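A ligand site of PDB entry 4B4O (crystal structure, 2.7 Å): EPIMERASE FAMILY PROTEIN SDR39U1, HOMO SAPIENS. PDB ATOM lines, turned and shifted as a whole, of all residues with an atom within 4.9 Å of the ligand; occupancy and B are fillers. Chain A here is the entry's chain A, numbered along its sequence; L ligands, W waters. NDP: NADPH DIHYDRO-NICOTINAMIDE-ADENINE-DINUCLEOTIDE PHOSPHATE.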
ATOM      1  N   GLY A   7      -4.237   5.019  29.651  1.00  0.00           N
ATOM      2  CA  GLY A   7      -4.041   6.426  30.001  1.00  0.00           C
ATOM      3  C   GLY A   7      -4.483   6.766  31.402  1.00  0.00           C
ATOM      4  O   GLY A   7      -4.654   7.944  31.743  1.00  0.00           O
ATOM      5  N   THR A   9      -2.991   7.021  34.213  1.00  0.00           N
ATOM      6  CA  THR A   9      -2.117   7.876  35.044  1.00  0.00           C
ATOM      7  C   THR A   9      -2.625   9.318  35.130  1.00  0.00           C
ATOM      8  O   THR A   9      -2.274  10.054  36.024  1.00  0.00           O
ATOM      9  CB  THR A   9      -0.678   7.937  34.491  1.00  0.00           C
ATOM     10  OG1 THR A   9      -0.701   8.300  33.106  1.00  0.00           O
ATOM     11  CG2 THR A   9       0.016   6.614  34.665  1.00  0.00           C
ATOM     12  N   GLY A  10      -3.492   9.698  34.191  1.00  0.00           N
ATOM     13  CA  GLY A  10      -3.910  11.091  34.048  1.00  0.00           C
ATOM     14  C   GLY A  10      -4.945  11.577  35.049  1.00  0.00           C
ATOM     15  O   GLY A  10      -5.173  10.964  36.106  1.00  0.00           O
ATOM     16  N   PHE A  11      -5.545  12.716  34.697  1.00  0.00           N
ATOM     17  CA  PHE A  11      -6.451  13.448  35.581  1.00  0.00           C
ATOM     18  C   PHE A  11      -7.714  12.654  35.844  1.00  0.00           C
ATOM     19  O   PHE A  11      -8.033  12.352  36.978  1.00  0.00           O
ATOM     20  CB  PHE A  11      -6.790  14.785  34.919  1.00  0.00           C
ATOM     21  CG  PHE A  11      -7.818  15.585  35.658  1.00  0.00           C
ATOM     22  CD1 PHE A  11      -7.634  15.910  36.996  1.00  0.00           C
ATOM     23  CD2 PHE A  11      -8.939  16.040  35.017  1.00  0.00           C
ATOM     24  CE1 PHE A  11      -8.552  16.678  37.670  1.00  0.00           C
ATOM     25  CE2 PHE A  11      -9.872  16.805  35.676  1.00  0.00           C
ATOM     26  CZ  PHE A  11      -9.685  17.119  37.006  1.00  0.00           C
ATOM     27  N   ILE A  12      -8.416  12.306  34.781  1.00  0.00           N
ATOM     28  CA  ILE A  12      -9.615  11.521  34.936  1.00  0.00           C
ATOM     29  C   ILE A  12      -9.250  10.136  35.475  1.00  0.00           C
ATOM     30  O   ILE A  12      -9.938   9.594  36.346  1.00  0.00           O
ATOM     31  CB  ILE A  12     -10.387  11.358  33.612  1.00  0.00           C
ATOM     32  CG1 ILE A  12     -10.901  12.712  33.090  1.00  0.00           C
ATOM     33  CG2 ILE A  12     -11.545  10.416  33.844  1.00  0.00           C
ATOM     34  CD1 ILE A  12     -11.315  12.751  31.616  1.00  0.00           C
ATOM     35  N   GLY A  13      -8.153   9.585  34.972  1.00  0.00           N
ATOM     36  CA  GLY A  13      -7.741   8.242  35.309  1.00  0.00           C
ATOM     37  C   GLY A  13      -7.461   8.029  36.782  1.00  0.00           C
ATOM     38  O   GLY A  13      -7.798   6.999  37.336  1.00  0.00           O
ATOM     39  N   VAL A  30      -2.633   1.104  31.516  1.00  0.00           N
ATOM     40  CA  VAL A  30      -1.758   1.075  30.348  1.00  0.00           C
ATOM     41  C   VAL A  30      -1.127   2.462  30.208  1.00  0.00           C
ATOM     42  O   VAL A  30      -1.828   3.466  30.265  1.00  0.00           O
ATOM     43  CB  VAL A  30      -2.469   0.685  29.031  1.00  0.00           C
ATOM     44  CG1 VAL A  30      -1.431   0.441  27.946  1.00  0.00           C
ATOM     45  CG2 VAL A  30      -3.289  -0.566  29.238  1.00  0.00           C
ATOM     46  N   SER A  31       0.186   2.497  30.062  1.00  0.00           N
ATOM     47  CA  SER A  31       0.929   3.749  30.095  1.00  0.00           C
ATOM     48  C   SER A  31       2.095   3.688  29.125  1.00  0.00           C
ATOM     49  O   SER A  31       2.545   2.611  28.759  1.00  0.00           O
ATOM     50  CB  SER A  31       1.446   3.977  31.527  1.00  0.00           C
ATOM     51  OG  SER A  31       2.351   5.057  31.595  1.00  0.00           O
ATOM     52  N   ARG A  32       2.586   4.857  28.723  1.00  0.00           N
ATOM     53  CA  ARG A  32       3.800   4.917  27.912  1.00  0.00           C
ATOM     54  C   ARG A  32       5.048   4.560  28.710  1.00  0.00           C
ATOM     55  O   ARG A  32       6.059   4.182  28.134  1.00  0.00           O
ATOM     56  CB  ARG A  32       3.976   6.290  27.312  1.00  0.00           C
ATOM     57  CG  ARG A  32       3.047   6.558  26.155  1.00  0.00           C
ATOM     58  CD  ARG A  32       3.068   8.022  25.768  1.00  0.00           C
ATOM     59  NE  ARG A  32       2.658   8.847  26.882  1.00  0.00           N
ATOM     60  CZ  ARG A  32       2.742  10.164  26.929  1.00  0.00           C
ATOM     61  NH1 ARG A  32       3.222  10.847  25.916  1.00  0.00           N
ATOM     62  NH2 ARG A  32       2.344  10.785  28.032  1.00  0.00           N
ATOM     63  N   LYS A  33       4.988   4.726  30.019  1.00  0.00           N
ATOM     64  CA  LYS A  33       6.141   4.503  30.885  1.00  0.00           C
ATOM     65  C   LYS A  33       5.831   3.334  31.816  1.00  0.00           C
ATOM     66  O   LYS A  33       4.724   3.252  32.368  1.00  0.00           O
ATOM     67  CB  LYS A  33       6.489   5.801  31.672  1.00  0.00           C
ATOM     68  CG  LYS A  33       7.723   6.609  31.196  1.00  0.00           C
ATOM     69  CD  LYS A  33       7.922   6.714  29.664  1.00  0.00           C
ATOM     70  CE  LYS A  33       9.224   7.407  29.258  1.00  0.00           C
ATOM     71  NZ  LYS A  33       9.594   7.061  27.854  1.00  0.00           N
ATOM     72  N   ARG A  38       0.894  -1.446  36.276  1.00  0.00           N
ATOM     73  CA  ARG A  38       0.685  -1.030  34.885  1.00  0.00           C
ATOM     74  C   ARG A  38       1.513  -1.802  33.862  1.00  0.00           C
ATOM     75  O   ARG A  38       2.530  -2.379  34.186  1.00  0.00           O
ATOM     76  CB  ARG A  38       0.976   0.458  34.735  1.00  0.00           C
ATOM     77  CG  ARG A  38       2.338   0.851  35.271  1.00  0.00           C
ATOM     78  CD  ARG A  38       2.677   2.286  34.963  1.00  0.00           C
ATOM     79  NE  ARG A  38       2.457   3.199  36.076  1.00  0.00           N
ATOM     80  CZ  ARG A  38       2.788   4.506  36.048  1.00  0.00           C
ATOM     81  NH1 ARG A  38       3.330   5.047  34.937  1.00  0.00           N
ATOM     82  NH2 ARG A  38       2.551   5.278  37.111  1.00  0.00           N
ATOM     83  N   TRP A  41       2.212   0.262  26.371  1.00  0.00           N
ATOM     84  CA  TRP A  41       1.583   0.051  25.048  1.00  0.00           C
ATOM     85  C   TRP A  41       2.345  -0.947  24.235  1.00  0.00           C
ATOM     86  O   TRP A  41       1.758  -1.824  23.609  1.00  0.00           O
ATOM     87  CB  TRP A  41       1.435   1.370  24.293  1.00  0.00           C
ATOM     88  CG  TRP A  41       0.479   2.286  25.020  1.00  0.00           C
ATOM     89  CD1 TRP A  41       0.806   3.364  25.839  1.00  0.00           C
ATOM     90  CD2 TRP A  41      -0.978   2.189  25.114  1.00  0.00           C
ATOM     91  NE1 TRP A  41      -0.308   3.931  26.388  1.00  0.00           N
ATOM     92  CE2 TRP A  41      -1.414   3.279  25.994  1.00  0.00           C
ATOM     93  CE3 TRP A  41      -1.932   1.352  24.562  1.00  0.00           C
ATOM     94  CZ2 TRP A  41      -2.744   3.500  26.281  1.00  0.00           C
ATOM     95  CZ3 TRP A  41      -3.270   1.585  24.866  1.00  0.00           C
ATOM     96  CH2 TRP A  41      -3.674   2.629  25.699  1.00  0.00           C
ATOM     97  N   LEU A  58      -8.554   6.214  28.270  1.00  0.00           N
ATOM     98  CA  LEU A  58      -8.507   7.656  28.543  1.00  0.00           C
ATOM     99  C   LEU A  58      -7.309   8.304  27.852  1.00  0.00           C
ATOM    100  O   LEU A  58      -7.095   9.522  27.966  1.00  0.00           O
ATOM    101  CB  LEU A  58      -8.410   7.900  30.054  1.00  0.00           C
ATOM    102  CG  LEU A  58      -9.496   7.270  30.919  1.00  0.00           C
ATOM    103  CD1 LEU A  58      -9.134   7.498  32.372  1.00  0.00           C
ATOM    104  CD2 LEU A  58     -10.854   7.829  30.610  1.00  0.00           C
ATOM    105  N   ALA A  59      -6.530   7.514  27.124  1.00  0.00           N
ATOM    106  CA  ALA A  59      -5.253   7.982  26.600  1.00  0.00           C
ATOM    107  C   ALA A  59      -5.453   9.098  25.566  1.00  0.00           C
ATOM    108  O   ALA A  59      -6.295   8.994  24.700  1.00  0.00           O
ATOM    109  CB  ALA A  59      -4.475   6.822  25.973  1.00  0.00           C
ATOM    110  N   GLY A  60      -4.641  10.155  25.670  1.00  0.00           N
ATOM    111  CA  GLY A  60      -4.660  11.234  24.682  1.00  0.00           C
ATOM    112  C   GLY A  60      -3.676  12.349  24.984  1.00  0.00           C
ATOM    113  O   GLY A  60      -3.551  12.780  26.129  1.00  0.00           O
ATOM    114  N   GLU A  61      -2.959  12.798  23.966  1.00  0.00           N
ATOM    115  CA  GLU A  61      -2.163  13.999  24.087  1.00  0.00           C
ATOM    116  C   GLU A  61      -3.090  15.135  24.529  1.00  0.00           C
ATOM    117  O   GLU A  61      -4.173  15.311  23.959  1.00  0.00           O
ATOM    118  CB  GLU A  61      -1.516  14.337  22.740  1.00  0.00           C
ATOM    119  CG  GLU A  61      -0.699  15.610  22.732  1.00  0.00           C
ATOM    120  CD  GLU A  61       0.675  15.481  23.362  1.00  0.00           C
ATOM    121  OE1 GLU A  61       1.093  14.371  23.745  1.00  0.00           O
ATOM    122  OE2 GLU A  61       1.339  16.535  23.469  1.00  0.00           O
ATOM    123  N   ASN A  62      -2.646  15.905  25.514  1.00  0.00           N
ATOM    124  CA  ASN A  62      -3.460  16.996  26.053  1.00  0.00           C
ATOM    125  C   ASN A  62      -3.738  18.132  25.054  1.00  0.00           C
ATOM    126  O   ASN A  62      -2.806  18.764  24.542  1.00  0.00           O
ATOM    127  CB  ASN A  62      -2.808  17.602  27.289  1.00  0.00           C
ATOM    128  CG  ASN A  62      -3.784  18.435  28.084  1.00  0.00           C
ATOM    129  OD1 ASN A  62      -3.833  19.652  27.960  1.00  0.00           O
ATOM    130  ND2 ASN A  62      -4.644  17.751  28.861  1.00  0.00           N
ATOM    131  N   ILE A  63      -5.017  18.382  24.802  1.00  0.00           N
ATOM    132  CA  ILE A  63      -5.419  19.305  23.758  1.00  0.00           C
ATOM    133  C   ILE A  63      -5.255  20.762  24.186  1.00  0.00           C
ATOM    134  O   ILE A  63      -4.690  21.569  23.451  1.00  0.00           O
ATOM    135  CB  ILE A  63      -6.887  19.056  23.358  1.00  0.00           C
ATOM    136  CG1 ILE A  63      -7.007  17.676  22.691  1.00  0.00           C
ATOM    137  CG2 ILE A  63      -7.398  20.139  22.416  1.00  0.00           C
ATOM    138  CD1 ILE A  63      -8.420  17.203  22.382  1.00  0.00           C
ATOM    139  N   SER A  81      -2.647   9.900  18.836  1.00  0.00           N
ATOM    140  CA  SER A  81      -2.590   9.372  20.190  1.00  0.00           C
ATOM    141  C   SER A  81      -3.912   8.719  20.606  1.00  0.00           C
ATOM    142  O   SER A  81      -3.915   7.736  21.319  1.00  0.00           O
ATOM    143  CB  SER A  81      -2.211  10.484  21.193  1.00  0.00           C
ATOM    144  OG  SER A  81      -3.230  11.471  21.325  1.00  0.00           O
ATOM    145  N   ARG A  82      -5.026   9.302  20.185  1.00  0.00           N
ATOM    146  CA  ARG A  82      -6.330   8.772  20.527  1.00  0.00           C
ATOM    147  C   ARG A  82      -6.728   7.557  19.658  1.00  0.00           C
ATOM    148  O   ARG A  82      -7.177   6.536  20.194  1.00  0.00           O
ATOM    149  CB  ARG A  82      -7.394   9.878  20.479  1.00  0.00           C
ATOM    150  CG  ARG A  82      -7.244  10.870  21.623  1.00  0.00           C
ATOM    151  CD  ARG A  82      -7.965  12.179  21.441  1.00  0.00           C
ATOM    152  NE  ARG A  82      -7.875  12.965  22.666  1.00  0.00           N
ATOM    153  CZ  ARG A  82      -6.888  13.798  22.985  1.00  0.00           C
ATOM    154  NH1 ARG A  82      -5.848  13.993  22.162  1.00  0.00           N
ATOM    155  NH2 ARG A  82      -6.935  14.439  24.141  1.00  0.00           N
ATOM    156  N   THR A  85      -4.013   4.322  20.330  1.00  0.00           N
ATOM    157  CA  THR A  85      -4.235   3.657  21.620  1.00  0.00           C
ATOM    158  C   THR A  85      -5.602   2.970  21.663  1.00  0.00           C
ATOM    159  O   THR A  85      -5.707   1.817  22.076  1.00  0.00           O
ATOM    160  CB  THR A  85      -4.120   4.596  22.833  1.00  0.00           C
ATOM    161  OG1 THR A  85      -5.107   5.622  22.747  1.00  0.00           O
ATOM    162  CG2 THR A  85      -2.714   5.184  22.911  1.00  0.00           C
ATOM    163  N   VAL A 106     -13.897   7.276  26.581  1.00  0.00           N
ATOM    164  CA  VAL A 106     -14.251   8.665  26.874  1.00  0.00           C
ATOM    165  C   VAL A 106     -13.912   9.473  25.649  1.00  0.00           C
ATOM    166  O   VAL A 106     -12.778   9.437  25.164  1.00  0.00           O
ATOM    167  CB  VAL A 106     -13.509   9.256  28.100  1.00  0.00           C
ATOM    168  CG1 VAL A 106     -13.655  10.767  28.150  1.00  0.00           C
ATOM    169  CG2 VAL A 106     -14.018   8.648  29.402  1.00  0.00           C
ATOM    170  N   THR A 107     -14.902  10.182  25.115  1.00  0.00           N
ATOM    171  CA  THR A 107     -14.651  11.186  24.078  1.00  0.00           C
ATOM    172  C   THR A 107     -15.257  12.501  24.562  1.00  0.00           C
ATOM    173  O   THR A 107     -15.239  12.781  25.776  1.00  0.00           O
ATOM    174  CB  THR A 107     -15.152  10.715  22.705  1.00  0.00           C
ATOM    175  OG1 THR A 107     -16.592  10.664  22.693  1.00  0.00           O
ATOM    176  CG2 THR A 107     -14.622   9.320  22.398  1.00  0.00           C
ATOM    177  N   GLY A 108     -15.767  13.337  23.663  1.00  0.00           N
ATOM    178  CA  GLY A 108     -16.122  14.697  24.035  1.00  0.00           C
ATOM    179  C   GLY A 108     -17.399  15.239  23.447  1.00  0.00           C
ATOM    180  O   GLY A 108     -17.875  14.775  22.422  1.00  0.00           O
ATOM    181  N   TRP A 139     -12.489   8.593  16.470  1.00  0.00           N
ATOM    182  CA  TRP A 139     -12.141   8.063  17.774  1.00  0.00           C
ATOM    183  C   TRP A 139     -13.106   6.976  18.197  1.00  0.00           C
ATOM    184  O   TRP A 139     -12.704   5.900  18.612  1.00  0.00           O
ATOM    185  CB  TRP A 139     -12.185   9.225  18.755  1.00  0.00           C
ATOM    186  CG  TRP A 139     -11.474   9.105  20.064  1.00  0.00           C
ATOM    187  CD1 TRP A 139     -10.812   8.011  20.602  1.00  0.00           C
ATOM    188  CD2 TRP A 139     -11.371  10.152  21.068  1.00  0.00           C
ATOM    189  NE1 TRP A 139     -10.311   8.329  21.846  1.00  0.00           N
ATOM    190  CE2 TRP A 139     -10.617   9.595  22.172  1.00  0.00           C
ATOM    191  CE3 TRP A 139     -11.804  11.457  21.143  1.00  0.00           C
ATOM    192  CZ2 TRP A 139     -10.338  10.322  23.298  1.00  0.00           C
ATOM    193  CZ3 TRP A 139     -11.511  12.179  22.296  1.00  0.00           C
ATOM    194  CH2 TRP A 139     -10.790  11.630  23.335  1.00  0.00           C
ATOM    195  N   SER A 157     -17.739  13.442  27.174  1.00  0.00           N
ATOM    196  CA  SER A 157     -17.601  14.258  28.368  1.00  0.00           C
ATOM    197  C   SER A 157     -17.595  15.758  28.078  1.00  0.00           C
ATOM    198  O   SER A 157     -17.045  16.225  27.075  1.00  0.00           O
ATOM    199  CB  SER A 157     -16.307  13.902  29.086  1.00  0.00           C
ATOM    200  OG  SER A 157     -16.148  14.630  30.289  1.00  0.00           O
ATOM    201  N   GLY A 158     -18.166  16.516  28.998  1.00  0.00           N
ATOM    202  CA  GLY A 158     -17.980  17.962  29.030  1.00  0.00           C
ATOM    203  C   GLY A 158     -16.698  18.282  29.783  1.00  0.00           C
ATOM    204  O   GLY A 158     -15.851  17.423  29.969  1.00  0.00           O
ATOM    205  N   VAL A 159     -16.536  19.550  30.171  1.00  0.00           N
ATOM    206  CA  VAL A 159     -15.336  20.003  30.857  1.00  0.00           C
ATOM    207  C   VAL A 159     -15.357  19.413  32.246  1.00  0.00           C
ATOM    208  O   VAL A 159     -16.333  19.566  32.981  1.00  0.00           O
ATOM    209  CB  VAL A 159     -15.318  21.531  30.981  1.00  0.00           C
ATOM    210  CG1 VAL A 159     -13.880  22.027  31.232  1.00  0.00           C
ATOM    211  CG2 VAL A 159     -15.891  22.124  29.689  1.00  0.00           C
ATOM    212  N   VAL A 160     -14.266  18.723  32.589  1.00  0.00           N
ATOM    213  CA  VAL A 160     -14.204  17.973  33.825  1.00  0.00           C
ATOM    214  C   VAL A 160     -13.598  18.861  34.881  1.00  0.00           C
ATOM    215  O   VAL A 160     -12.431  19.225  34.781  1.00  0.00           O
ATOM    216  CB  VAL A 160     -13.353  16.700  33.652  1.00  0.00           C
ATOM    217  CG1 VAL A 160     -13.472  15.878  34.922  1.00  0.00           C
ATOM    218  CG2 VAL A 160     -13.728  15.960  32.368  1.00  0.00           C
HETATM  219  PA  NDP L   1      -4.781  13.734  30.885  1.00  0.00           P
HETATM  220  O1A NDP L   1      -3.922  14.545  29.888  1.00  0.00           O
HETATM  221  O2A NDP L   1      -4.703  14.018  32.406  1.00  0.00           O
HETATM  222  O5B NDP L   1      -4.453  12.138  30.834  1.00  0.00           O
HETATM  223  C5B NDP L   1      -4.049  11.614  29.571  1.00  0.00           C
HETATM  224  C4B NDP L   1      -3.199  10.397  29.806  1.00  0.00           C
HETATM  225  O4B NDP L   1      -2.983   9.775  28.546  1.00  0.00           O
HETATM  226  C3B NDP L   1      -1.834  10.761  30.410  1.00  0.00           C
HETATM  227  O3B NDP L   1      -1.724  10.462  31.827  1.00  0.00           O
HETATM  228  C2B NDP L   1      -0.845   9.899  29.624  1.00  0.00           C
HETATM  229  O2B NDP L   1      -0.540   8.694  30.300  1.00  0.00           O
HETATM  230  C1B NDP L   1      -1.604   9.518  28.386  1.00  0.00           C
HETATM  231  N9A NDP L   1      -1.075  10.359  27.316  1.00  0.00           N
HETATM  232  C8A NDP L   1      -0.808  11.708  27.271  1.00  0.00           C
HETATM  233  N7A NDP L   1      -0.259  12.012  26.013  1.00  0.00           N
HETATM  234  C5A NDP L   1      -0.206  10.863  25.299  1.00  0.00           C
HETATM  235  C6A NDP L   1       0.219  10.440  23.956  1.00  0.00           C
HETATM  236  N6A NDP L   1       0.686  11.324  23.061  1.00  0.00           N
HETATM  237  N1A NDP L   1       0.118   9.137  23.625  1.00  0.00           N
HETATM  238  C2A NDP L   1      -0.353   8.235  24.541  1.00  0.00           C
HETATM  239  N3A NDP L   1      -0.792   8.549  25.777  1.00  0.00           N
HETATM  240  C4A NDP L   1      -0.743   9.795  26.162  1.00  0.00           C
HETATM  241  O3  NDP L   1      -6.266  13.927  30.273  1.00  0.00           O
HETATM  242  PN  NDP L   1      -7.622  13.791  31.131  1.00  0.00           P
HETATM  243  O1N NDP L   1      -7.400  12.757  32.225  1.00  0.00           O
HETATM  244  O2N NDP L   1      -8.093  15.146  31.538  1.00  0.00           O
HETATM  245  O5D NDP L   1      -8.673  13.217  30.000  1.00  0.00           O
HETATM  246  C5D NDP L   1      -8.378  11.901  29.497  1.00  0.00           C
HETATM  247  C4D NDP L   1      -9.073  11.625  28.181  1.00  0.00           C
HETATM  248  O4D NDP L   1     -10.372  12.180  28.318  1.00  0.00           O
HETATM  249  C3D NDP L   1      -8.440  12.307  26.954  1.00  0.00           C
HETATM  250  O3D NDP L   1      -8.493  11.432  25.786  1.00  0.00           O
HETATM  251  C2D NDP L   1      -9.273  13.585  26.771  1.00  0.00           C
HETATM  252  O2D NDP L   1      -9.517  14.049  25.436  1.00  0.00           O
HETATM  253  C1D NDP L   1     -10.622  13.148  27.277  1.00  0.00           C
HETATM  254  N1N NDP L   1     -11.455  14.260  27.764  1.00  0.00           N
HETATM  255  C2N NDP L   1     -11.049  15.067  28.752  1.00  0.00           C
HETATM  256  C3N NDP L   1     -11.844  16.103  29.188  1.00  0.00           C
HETATM  257  C7N NDP L   1     -11.345  16.959  30.297  1.00  0.00           C
HETATM  258  O7N NDP L   1     -10.411  16.543  30.976  1.00  0.00           O
HETATM  259  N7N NDP L   1     -11.899  18.148  30.539  1.00  0.00           N
HETATM  260  C4N NDP L   1     -13.204  16.328  28.635  1.00  0.00           C
HETATM  261  C5N NDP L   1     -13.560  15.383  27.586  1.00  0.00           C
HETATM  262  C6N NDP L   1     -12.670  14.384  27.199  1.00  0.00           C
HETATM  263  P2B NDP L   1       1.029   8.161  30.336  1.00  0.00           P
HETATM  264  O1X NDP L   1       1.297   7.566  28.963  1.00  0.00           O
HETATM  265  O2X NDP L   1       1.932   9.400  30.638  1.00  0.00           O
HETATM  266  O3X NDP L   1       0.839   7.116  31.463  1.00  0.00           O
HETATM  267  O   HOH W   1      -1.483   5.971  31.914  1.00  0.00           O
HETATM  268  O   HOH W   2      -5.086  14.772  27.359  1.00  0.00           O
HETATM  269  O   HOH W   3      -6.346  10.234  32.572  1.00  0.00           O
HETATM  270  O   HOH W   4     -10.410   8.629  26.006  1.00  0.00           O
HETATM  271  O   HOH W   5      -1.811  14.331  33.725  1.00  0.00           O
HETATM  272  O   HOH W   6      -7.163  16.404  26.103  1.00  0.00           O
HETATM  273  O   HOH W   7      -0.099  12.205  32.828  1.00  0.00           O
HETATM  274  O   HOH W   8      -0.542   6.593  27.757  1.00  0.00           O
HETATM  275  O   HOH W   9      -6.169  17.134  31.427  1.00  0.00           O
HETATM  276  O   HOH W  10     -10.820  19.424  32.597  1.00  0.00           O
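The side-chain hydroxyl (OG) of Ser 31 sits at hydrogen-bond distance from the guanidinium group (NH1) of Arg 38, at 3.5 Å. The backbone carbonyl oxygen of Thr 107 is in hydrogen-bond range of the backbone NH of Ser 157, 2.9 Å away. The side-chain hydroxyl (OG) of Ser 31 is in hydrogen-bond range of the backbone carbonyl oxygen (O) of Lys 33 (3.1 Å). The backbone carbonyl oxygen of Glu 61 sits at hydrogen-bond distance from the guanidinium group of Arg 82, 2.8 Å away. The backbone NH (N) of Gly 7 is in hydrogen-bond range of the backbone carbonyl oxygen (O) of Val 30. The backbone NH (N) of Glu 61 is in hydrogen-bond range of the side-chain hydroxyl (OG) of Ser 81 (3.0 Å). The backbone carbonyl oxygen (O) of Ser 31 lies within hydrogen-bond range of the backbone NH (N) of Trp 41. The backbone carbonyl oxygen of Ser 81 is in hydrogen-bond range of the side-chain hydroxyl of Thr 85, at 2.8 Å.
N of Glu 61 lies close to N7A of the ligand. O3B of the ligand sits at hydrogen-bond distance from N of Gly 10. NH2 of Arg 82 sits at hydrogen-bond distance from O2D of the ligand (2.9 Å). An oxygen (O3X) of the ligand lies within hydrogen-bond range of the side-chain hydroxyl of Ser 31, at 2.6 Å. The backbone NH (N) of Phe 11 lies within hydrogen-bond range of an oxygen (O2A) of the ligand (2.8 Å). The guanidinium group (NE) of Arg 32 lies within salt-bridge range of an oxygen (O1X) of the ligand. O of Ala 59 lies within hydrogen-bond range of O3D of the ligand. The backbone NH (N) of Arg 32 sits at hydrogen-bond distance from an oxygen (O1X) of the ligand, at 3.0 Å. A nitrogen (N6A) of the ligand is in hydrogen-bond range of the side-chain carboxylate (OE1) of Glu 61 (3.1 Å). The backbone NH (N) of Gly 60 lies within hydrogen-bond range of an oxygen (O4B) of the ligand, at 3.3 Å. An oxygen (O3D) of the ligand sits close to the backbone carbonyl oxygen (O) of Leu 58. An oxygen (O1N) of the ligand sits at hydrogen-bond distance from the backbone NH of Ile 12, 2.8 Å away. The side-chain hydroxyl (OG1) of Thr 9 is in hydrogen-bond range of an oxygen (O3X) of the ligand (2.5 Å). The side-chain amide nitrogen (ND2) of Asn 62 is in hydrogen-bond range of an oxygen (O1A) of the ligand, at 3.4 Å.
Water W8 lies within hydrogen-bond range of an oxygen (O1X) of the ligand (2.4 Å) and the indole nitrogen (NE1) of Trp 41 (3.0 Å). Water W1 lies within hydrogen-bond range of an oxygen (O3X) of the ligand (2.6 Å), the side-chain hydroxyl (OG1) of Thr 9 (2.7 Å) and the backbone carbonyl oxygen (O) of Val 30 (3.0 Å). Water W10 bridges a nitrogen (N7N) of the ligand (2.7 Å) and the backbone carbonyl oxygen of Val 160 (2.7 Å). Water W9 lies within hydrogen-bond range of an oxygen (O2N) of the ligand (2.8 Å) and the side-chain amide nitrogen (ND2) of Asn 62 (3.0 Å). Water W2 lies within hydrogen-bond range of an oxygen (O1A) of the ligand, the backbone carbonyl oxygen of Gly 60 and the backbone NH of Asn 62. Water W4 bridges O of Val 106 and O3D of the ligand.
The backbone NH (N) of Val 160 lies close to a nitrogen (N7N) of the ligand, at 3.2 Å. Residues that only touch the ligand: Gly 7 (3.4 Å), Ser 81 (3.5 Å), Val 106 (3.6 Å), Thr 107 (3.3 Å), Trp 139 (3.3 Å), Ser 157 (3.5 Å), Gly 158 (3.2 Å) and Val 159 (3.9 Å). 21 residues have an atom within 4 Å of the ligand: Gly 7, Thr 9, Gly 10, Phe 11, Ile 12, Ser 31, Arg 32, Leu 58, Ala 59, Gly 60, Glu 61, Asn 62, Ser 81, Arg 82, Val 106, Thr 107, Trp 139, Ser 157, Gly 158, Val 159 and Val 160.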
